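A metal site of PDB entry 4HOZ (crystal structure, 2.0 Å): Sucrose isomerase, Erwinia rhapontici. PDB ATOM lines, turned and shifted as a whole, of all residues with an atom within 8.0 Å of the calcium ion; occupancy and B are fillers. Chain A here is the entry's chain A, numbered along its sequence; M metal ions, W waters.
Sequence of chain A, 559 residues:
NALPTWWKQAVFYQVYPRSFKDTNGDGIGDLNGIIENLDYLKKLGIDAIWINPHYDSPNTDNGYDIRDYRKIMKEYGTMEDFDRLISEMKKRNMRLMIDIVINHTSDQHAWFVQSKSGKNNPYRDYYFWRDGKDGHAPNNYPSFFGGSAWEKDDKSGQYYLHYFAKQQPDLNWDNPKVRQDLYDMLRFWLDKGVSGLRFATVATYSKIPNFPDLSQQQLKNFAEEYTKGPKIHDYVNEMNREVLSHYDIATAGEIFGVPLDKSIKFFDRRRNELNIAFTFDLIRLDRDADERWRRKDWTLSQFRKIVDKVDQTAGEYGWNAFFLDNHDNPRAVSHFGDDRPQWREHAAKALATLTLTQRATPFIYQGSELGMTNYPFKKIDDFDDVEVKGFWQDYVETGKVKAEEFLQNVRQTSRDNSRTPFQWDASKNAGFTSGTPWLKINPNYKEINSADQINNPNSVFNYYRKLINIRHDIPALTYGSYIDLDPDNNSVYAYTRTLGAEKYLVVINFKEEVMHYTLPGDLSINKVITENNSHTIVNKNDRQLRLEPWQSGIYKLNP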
ATOM      1  N   PRO A  17      31.675 -28.624  17.058  1.00  0.00           N
ATOM      2  CA  PRO A  17      30.248 -28.976  16.974  1.00  0.00           C
ATOM      3  C   PRO A  17      29.646 -28.873  15.553  1.00  0.00           C
ATOM      4  O   PRO A  17      28.931 -29.734  15.139  1.00  0.00           O
ATOM      5  CB  PRO A  17      29.591 -27.994  17.954  1.00  0.00           C
ATOM      6  CG  PRO A  17      30.660 -27.781  19.004  1.00  0.00           C
ATOM      7  CD  PRO A  17      31.941 -27.657  18.163  1.00  0.00           C
ATOM      8  N   ARG A  18      30.076 -27.873  14.785  1.00  0.00           N
ATOM      9  CA  ARG A  18      29.581 -27.684  13.418  1.00  0.00           C
ATOM     10  C   ARG A  18      29.686 -28.944  12.529  1.00  0.00           C
ATOM     11  O   ARG A  18      28.886 -29.129  11.596  1.00  0.00           O
ATOM     12  CB  ARG A  18      30.409 -26.569  12.790  1.00  0.00           C
ATOM     13  CG  ARG A  18      29.757 -25.873  11.615  1.00  0.00           C
ATOM     14  CD  ARG A  18      30.640 -24.678  11.137  1.00  0.00           C
ATOM     15  NE  ARG A  18      30.072 -24.298   9.880  1.00  0.00           N
ATOM     16  CZ  ARG A  18      29.027 -23.487   9.747  1.00  0.00           C
ATOM     17  NH1 ARG A  18      28.512 -22.835  10.785  1.00  0.00           N
ATOM     18  NH2 ARG A  18      28.563 -23.254   8.553  1.00  0.00           N
ATOM     19  N   LYS A  21      27.870 -33.953  14.626  1.00  0.00           N
ATOM     20  CA  LYS A  21      26.662 -34.741  14.259  1.00  0.00           C
ATOM     21  C   LYS A  21      25.483 -33.783  14.166  1.00  0.00           C
ATOM     22  O   LYS A  21      25.178 -33.069  15.137  1.00  0.00           O
ATOM     23  CB  LYS A  21      26.347 -35.826  15.329  1.00  0.00           C
ATOM     24  CG  LYS A  21      25.058 -36.666  15.120  1.00  0.00           C
ATOM     25  CD  LYS A  21      25.120 -37.451  13.819  1.00  0.00           C
ATOM     26  CE  LYS A  21      23.716 -37.827  13.275  1.00  0.00           C
ATOM     27  NZ  LYS A  21      23.530 -39.208  13.720  1.00  0.00           N
ATOM     28  N   ASP A  22      24.796 -33.793  13.013  1.00  0.00           N
ATOM     29  CA  ASP A  22      23.613 -33.009  12.751  1.00  0.00           C
ATOM     30  C   ASP A  22      22.389 -33.863  13.157  1.00  0.00           C
ATOM     31  O   ASP A  22      22.211 -34.962  12.620  1.00  0.00           O
ATOM     32  CB  ASP A  22      23.578 -32.736  11.241  1.00  0.00           C
ATOM     33  CG  ASP A  22      22.301 -32.065  10.784  1.00  0.00           C
ATOM     34  OD1 ASP A  22      21.568 -31.605  11.681  1.00  0.00           O
ATOM     35  OD2 ASP A  22      22.031 -31.969   9.558  1.00  0.00           O
ATOM     36  N   THR A  23      21.564 -33.393  14.073  1.00  0.00           N
ATOM     37  CA  THR A  23      20.349 -34.179  14.442  1.00  0.00           C
ATOM     38  C   THR A  23      19.056 -33.548  13.889  1.00  0.00           C
ATOM     39  O   THR A  23      17.960 -33.988  14.236  1.00  0.00           O
ATOM     40  CB  THR A  23      20.224 -34.353  15.959  1.00  0.00           C
ATOM     41  OG1 THR A  23      20.192 -33.082  16.566  1.00  0.00           O
ATOM     42  CG2 THR A  23      21.419 -35.181  16.518  1.00  0.00           C
ATOM     43  N   ASN A  24      19.132 -32.502  13.073  1.00  0.00           N
ATOM     44  CA  ASN A  24      17.841 -31.984  12.555  1.00  0.00           C
ATOM     45  C   ASN A  24      17.849 -31.709  11.062  1.00  0.00           C
ATOM     46  O   ASN A  24      16.961 -31.039  10.566  1.00  0.00           O
ATOM     47  CB  ASN A  24      17.366 -30.744  13.336  1.00  0.00           C
ATOM     48  CG  ASN A  24      18.412 -29.638  13.319  1.00  0.00           C
ATOM     49  OD1 ASN A  24      19.242 -29.572  12.431  1.00  0.00           O
ATOM     50  ND2 ASN A  24      18.390 -28.785  14.305  1.00  0.00           N
ATOM     51  N   GLY A  25      18.865 -32.168  10.347  1.00  0.00           N
ATOM     52  CA  GLY A  25      18.829 -32.183   8.908  1.00  0.00           C
ATOM     53  C   GLY A  25      19.159 -30.882   8.211  1.00  0.00           C
ATOM     54  O   GLY A  25      19.118 -30.839   6.979  1.00  0.00           O
ATOM     55  N   ASP A  26      19.574 -29.841   8.950  1.00  0.00           N
ATOM     56  CA  ASP A  26      19.972 -28.607   8.303  1.00  0.00           C
ATOM     57  C   ASP A  26      21.435 -28.681   7.786  1.00  0.00           C
ATOM     58  O   ASP A  26      21.937 -27.709   7.250  1.00  0.00           O
ATOM     59  CB  ASP A  26      19.740 -27.383   9.219  1.00  0.00           C
ATOM     60  CG  ASP A  26      20.727 -27.365  10.462  1.00  0.00           C
ATOM     61  OD1 ASP A  26      21.616 -28.322  10.606  1.00  0.00           O
ATOM     62  OD2 ASP A  26      20.682 -26.382  11.225  1.00  0.00           O
ATOM     63  N   GLY A  27      22.094 -29.801   7.886  1.00  0.00           N
ATOM     64  CA  GLY A  27      23.487 -29.916   7.420  1.00  0.00           C
ATOM     65  C   GLY A  27      24.618 -29.506   8.390  1.00  0.00           C
ATOM     66  O   GLY A  27      25.791 -29.621   8.057  1.00  0.00           O
ATOM     67  N   ILE A  28      24.261 -29.028   9.585  1.00  0.00           N
ATOM     68  CA  ILE A  28      25.203 -28.432  10.528  1.00  0.00           C
ATOM     69  C   ILE A  28      25.133 -29.220  11.830  1.00  0.00           C
ATOM     70  O   ILE A  28      24.061 -29.519  12.345  1.00  0.00           O
ATOM     71  CB  ILE A  28      24.865 -26.934  10.778  1.00  0.00           C
ATOM     72  CG1 ILE A  28      25.185 -26.127   9.524  1.00  0.00           C
ATOM     73  CG2 ILE A  28      25.706 -26.321  11.913  1.00  0.00           C
ATOM     74  CD1 ILE A  28      24.591 -24.716   9.624  1.00  0.00           C
ATOM     75  N   GLY A  29      26.276 -29.613  12.357  1.00  0.00           N
ATOM     76  CA  GLY A  29      26.250 -30.302  13.630  1.00  0.00           C
ATOM     77  C   GLY A  29      25.697 -29.424  14.713  1.00  0.00           C
ATOM     78  O   GLY A  29      25.660 -28.173  14.590  1.00  0.00           O
ATOM     79  N   ASP A  30      25.245 -30.054  15.802  1.00  0.00           N
ATOM     80  CA  ASP A  30      24.518 -29.278  16.832  1.00  0.00           C
ATOM     81  C   ASP A  30      24.726 -29.911  18.191  1.00  0.00           C
ATOM     82  O   ASP A  30      25.248 -30.996  18.269  1.00  0.00           O
ATOM     83  CB  ASP A  30      23.012 -29.203  16.468  1.00  0.00           C
ATOM     84  CG  ASP A  30      22.442 -30.529  16.112  1.00  0.00           C
ATOM     85  OD1 ASP A  30      22.351 -31.431  16.991  1.00  0.00           O
ATOM     86  OD2 ASP A  30      22.067 -30.716  14.930  1.00  0.00           O
ATOM     87  N   LEU A  31      24.309 -29.263  19.283  1.00  0.00           N
ATOM     88  CA  LEU A  31      24.491 -29.813  20.639  1.00  0.00           C
ATOM     89  C   LEU A  31      23.838 -31.178  20.891  1.00  0.00           C
ATOM     90  O   LEU A  31      24.460 -32.119  21.448  1.00  0.00           O
ATOM     91  CB  LEU A  31      24.009 -28.793  21.676  1.00  0.00           C
ATOM     92  CG  LEU A  31      24.792 -27.505  21.730  1.00  0.00           C
ATOM     93  CD1 LEU A  31      24.207 -26.620  22.813  1.00  0.00           C
ATOM     94  CD2 LEU A  31      26.278 -27.784  22.010  1.00  0.00           C
ATOM     95  N   ASN A  32      22.561 -31.318  20.478  1.00  0.00           N
ATOM     96  CA  ASN A  32      21.937 -32.639  20.495  1.00  0.00           C
ATOM     97  C   ASN A  32      22.777 -33.755  19.823  1.00  0.00           C
ATOM     98  O   ASN A  32      22.811 -34.889  20.290  1.00  0.00           O
ATOM     99  CB  ASN A  32      20.528 -32.572  19.930  1.00  0.00           C
ATOM    100  CG  ASN A  32      19.595 -31.810  20.886  1.00  0.00           C
ATOM    101  OD1 ASN A  32      19.891 -31.705  22.088  1.00  0.00           O
ATOM    102  ND2 ASN A  32      18.475 -31.272  20.373  1.00  0.00           N
ATOM    103  N   GLY A  33      23.426 -33.446  18.732  1.00  0.00           N
ATOM    104  CA  GLY A  33      24.317 -34.465  18.128  1.00  0.00           C
ATOM    105  C   GLY A  33      25.453 -34.815  19.052  1.00  0.00           C
ATOM    106  O   GLY A  33      25.893 -35.946  19.009  1.00  0.00           O
ATOM    107  N   LYS A  74      22.488 -20.212  17.333  1.00  0.00           N
ATOM    108  CA  LYS A  74      21.184 -20.651  16.897  1.00  0.00           C
ATOM    109  C   LYS A  74      21.300 -22.050  16.214  1.00  0.00           C
ATOM    110  O   LYS A  74      20.522 -22.920  16.515  1.00  0.00           O
ATOM    111  CB  LYS A  74      20.580 -19.618  15.939  1.00  0.00           C
ATOM    112  CG  LYS A  74      19.201 -20.034  15.359  1.00  0.00           C
ATOM    113  CD  LYS A  74      18.779 -19.162  14.161  1.00  0.00           C
ATOM    114  CE  LYS A  74      19.919 -18.280  13.609  1.00  0.00           C
ATOM    115  NZ  LYS A  74      20.454 -18.553  12.223  1.00  0.00           N
ATOM    116  N   GLU A  75      22.322 -22.250  15.358  1.00  0.00           N
ATOM    117  CA  GLU A  75      22.567 -23.523  14.688  1.00  0.00           C
ATOM    118  C   GLU A  75      22.886 -24.723  15.588  1.00  0.00           C
ATOM    119  O   GLU A  75      22.763 -25.860  15.118  1.00  0.00           O
ATOM    120  CB  GLU A  75      23.678 -23.390  13.649  1.00  0.00           C
ATOM    121  CG  GLU A  75      23.345 -22.522  12.453  1.00  0.00           C
ATOM    122  CD  GLU A  75      23.600 -21.041  12.643  1.00  0.00           C
ATOM    123  OE1 GLU A  75      23.967 -20.539  13.758  1.00  0.00           O
ATOM    124  OE2 GLU A  75      23.477 -20.348  11.624  1.00  0.00           O
ATOM    125  N   TYR A  76      23.287 -24.467  16.840  1.00  0.00           N
ATOM    126  CA  TYR A  76      23.677 -25.568  17.747  1.00  0.00           C
ATOM    127  C   TYR A  76      22.573 -25.941  18.703  1.00  0.00           C
ATOM    128  O   TYR A  76      22.584 -27.034  19.287  1.00  0.00           O
ATOM    129  CB  TYR A  76      24.968 -25.259  18.536  1.00  0.00           C
ATOM    130  CG  TYR A  76      26.224 -25.107  17.672  1.00  0.00           C
ATOM    131  CD1 TYR A  76      26.249 -25.469  16.307  1.00  0.00           C
ATOM    132  CD2 TYR A  76      27.346 -24.541  18.202  1.00  0.00           C
ATOM    133  CE1 TYR A  76      27.396 -25.317  15.504  1.00  0.00           C
ATOM    134  CE2 TYR A  76      28.483 -24.347  17.431  1.00  0.00           C
ATOM    135  CZ  TYR A  76      28.518 -24.717  16.098  1.00  0.00           C
ATOM    136  OH  TYR A  76      29.675 -24.446  15.430  1.00  0.00           O
ATOM    137  N   GLY A  77      21.593 -25.066  18.868  1.00  0.00           N
ATOM    138  CA  GLY A  77      20.493 -25.400  19.801  1.00  0.00           C
ATOM    139  C   GLY A  77      20.172 -24.261  20.757  1.00  0.00           C
ATOM    140  O   GLY A  77      20.327 -23.077  20.401  1.00  0.00           O
ATOM    141  N   PHE A 432      26.136 -38.534   8.940  1.00  0.00           N
ATOM    142  CA  PHE A 432      26.345 -37.268   9.661  1.00  0.00           C
ATOM    143  C   PHE A 432      25.043 -36.433   9.673  1.00  0.00           C
ATOM    144  O   PHE A 432      24.791 -35.712  10.629  1.00  0.00           O
ATOM    145  CB  PHE A 432      27.475 -36.481   8.978  1.00  0.00           C
ATOM    146  CG  PHE A 432      27.521 -35.027   9.378  1.00  0.00           C
ATOM    147  CD1 PHE A 432      28.039 -34.624  10.638  1.00  0.00           C
ATOM    148  CD2 PHE A 432      27.028 -34.038   8.523  1.00  0.00           C
ATOM    149  CE1 PHE A 432      28.006 -33.256  11.007  1.00  0.00           C
ATOM    150  CE2 PHE A 432      27.007 -32.685   8.903  1.00  0.00           C
ATOM    151  CZ  PHE A 432      27.544 -32.287  10.125  1.00  0.00           C
ATOM    152  N   THR A 433      24.260 -36.488   8.578  1.00  0.00           N
ATOM    153  CA  THR A 433      23.141 -35.622   8.395  1.00  0.00           C
ATOM    154  C   THR A 433      22.113 -36.348   7.530  1.00  0.00           C
ATOM    155  O   THR A 433      22.478 -37.237   6.735  1.00  0.00           O
ATOM    156  CB  THR A 433      23.545 -34.310   7.702  1.00  0.00           C
ATOM    157  OG1 THR A 433      22.399 -33.495   7.528  1.00  0.00           O
ATOM    158  CG2 THR A 433      24.207 -34.534   6.317  1.00  0.00           C
HETATM  159 CA    CA M   1      21.711 -29.437  12.804  1.00  0.00          CA
HETATM  160  O   HOH W   1      21.252 -27.290  13.739  1.00  0.00           O
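The side-chain carboxylate of Asp 22 lies within hydrogen-bond range of the backbone NH of Gly 25 (3.3 Å).
The side-chain carboxylate of Asp 30 sits at hydrogen-bond distance from the backbone NH of Gly 33 (2.9 Å).
The side-chain carboxylate of Asp 22 lies within hydrogen-bond range of the backbone NH of Gly 27, 2.7 Å away.
The backbone carbonyl oxygen (O) of Phe 432 lies within hydrogen-bond range of the backbone NH (N) of Asp 22 (3.1 Å).
The backbone NH of Asp 30 sits at hydrogen-bond distance from the backbone carbonyl oxygen of Lys 21 (3.1 Å).
The side-chain carboxylate (OD1) of Asp 30 sits close to the backbone NH (N) of Asn 32, 3.5 Å away.
The side-chain hydroxyl of Thr 433 lies within hydrogen-bond range of the side-chain carboxylate of Asp 22, at 2.6 Å.
OD1 of Asp 30 lies within hydrogen-bond range of OG1 of Thr 23.
Of the 21 residues printed, 5 come within 4 Å of the calcium ion.
Along chain A the residues within 4 Å of the calcium ion span positions 22 to 30.
The nearest printed residue that does not touch the calcium ion is Thr 23 (4.2 Å).
The calcium ion is bound by water W1, O of Ile 28, OD1 of Asp 22, OD1 of Asp 26, OD1 of Asn 24 and OD2 of Asp 30.
The calcium ion has six donor atoms within binding distance.
Water W1 lies within hydrogen-bond range of O of Glu 75, OD2 of Asp 26 and ND2 of Asn 24.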
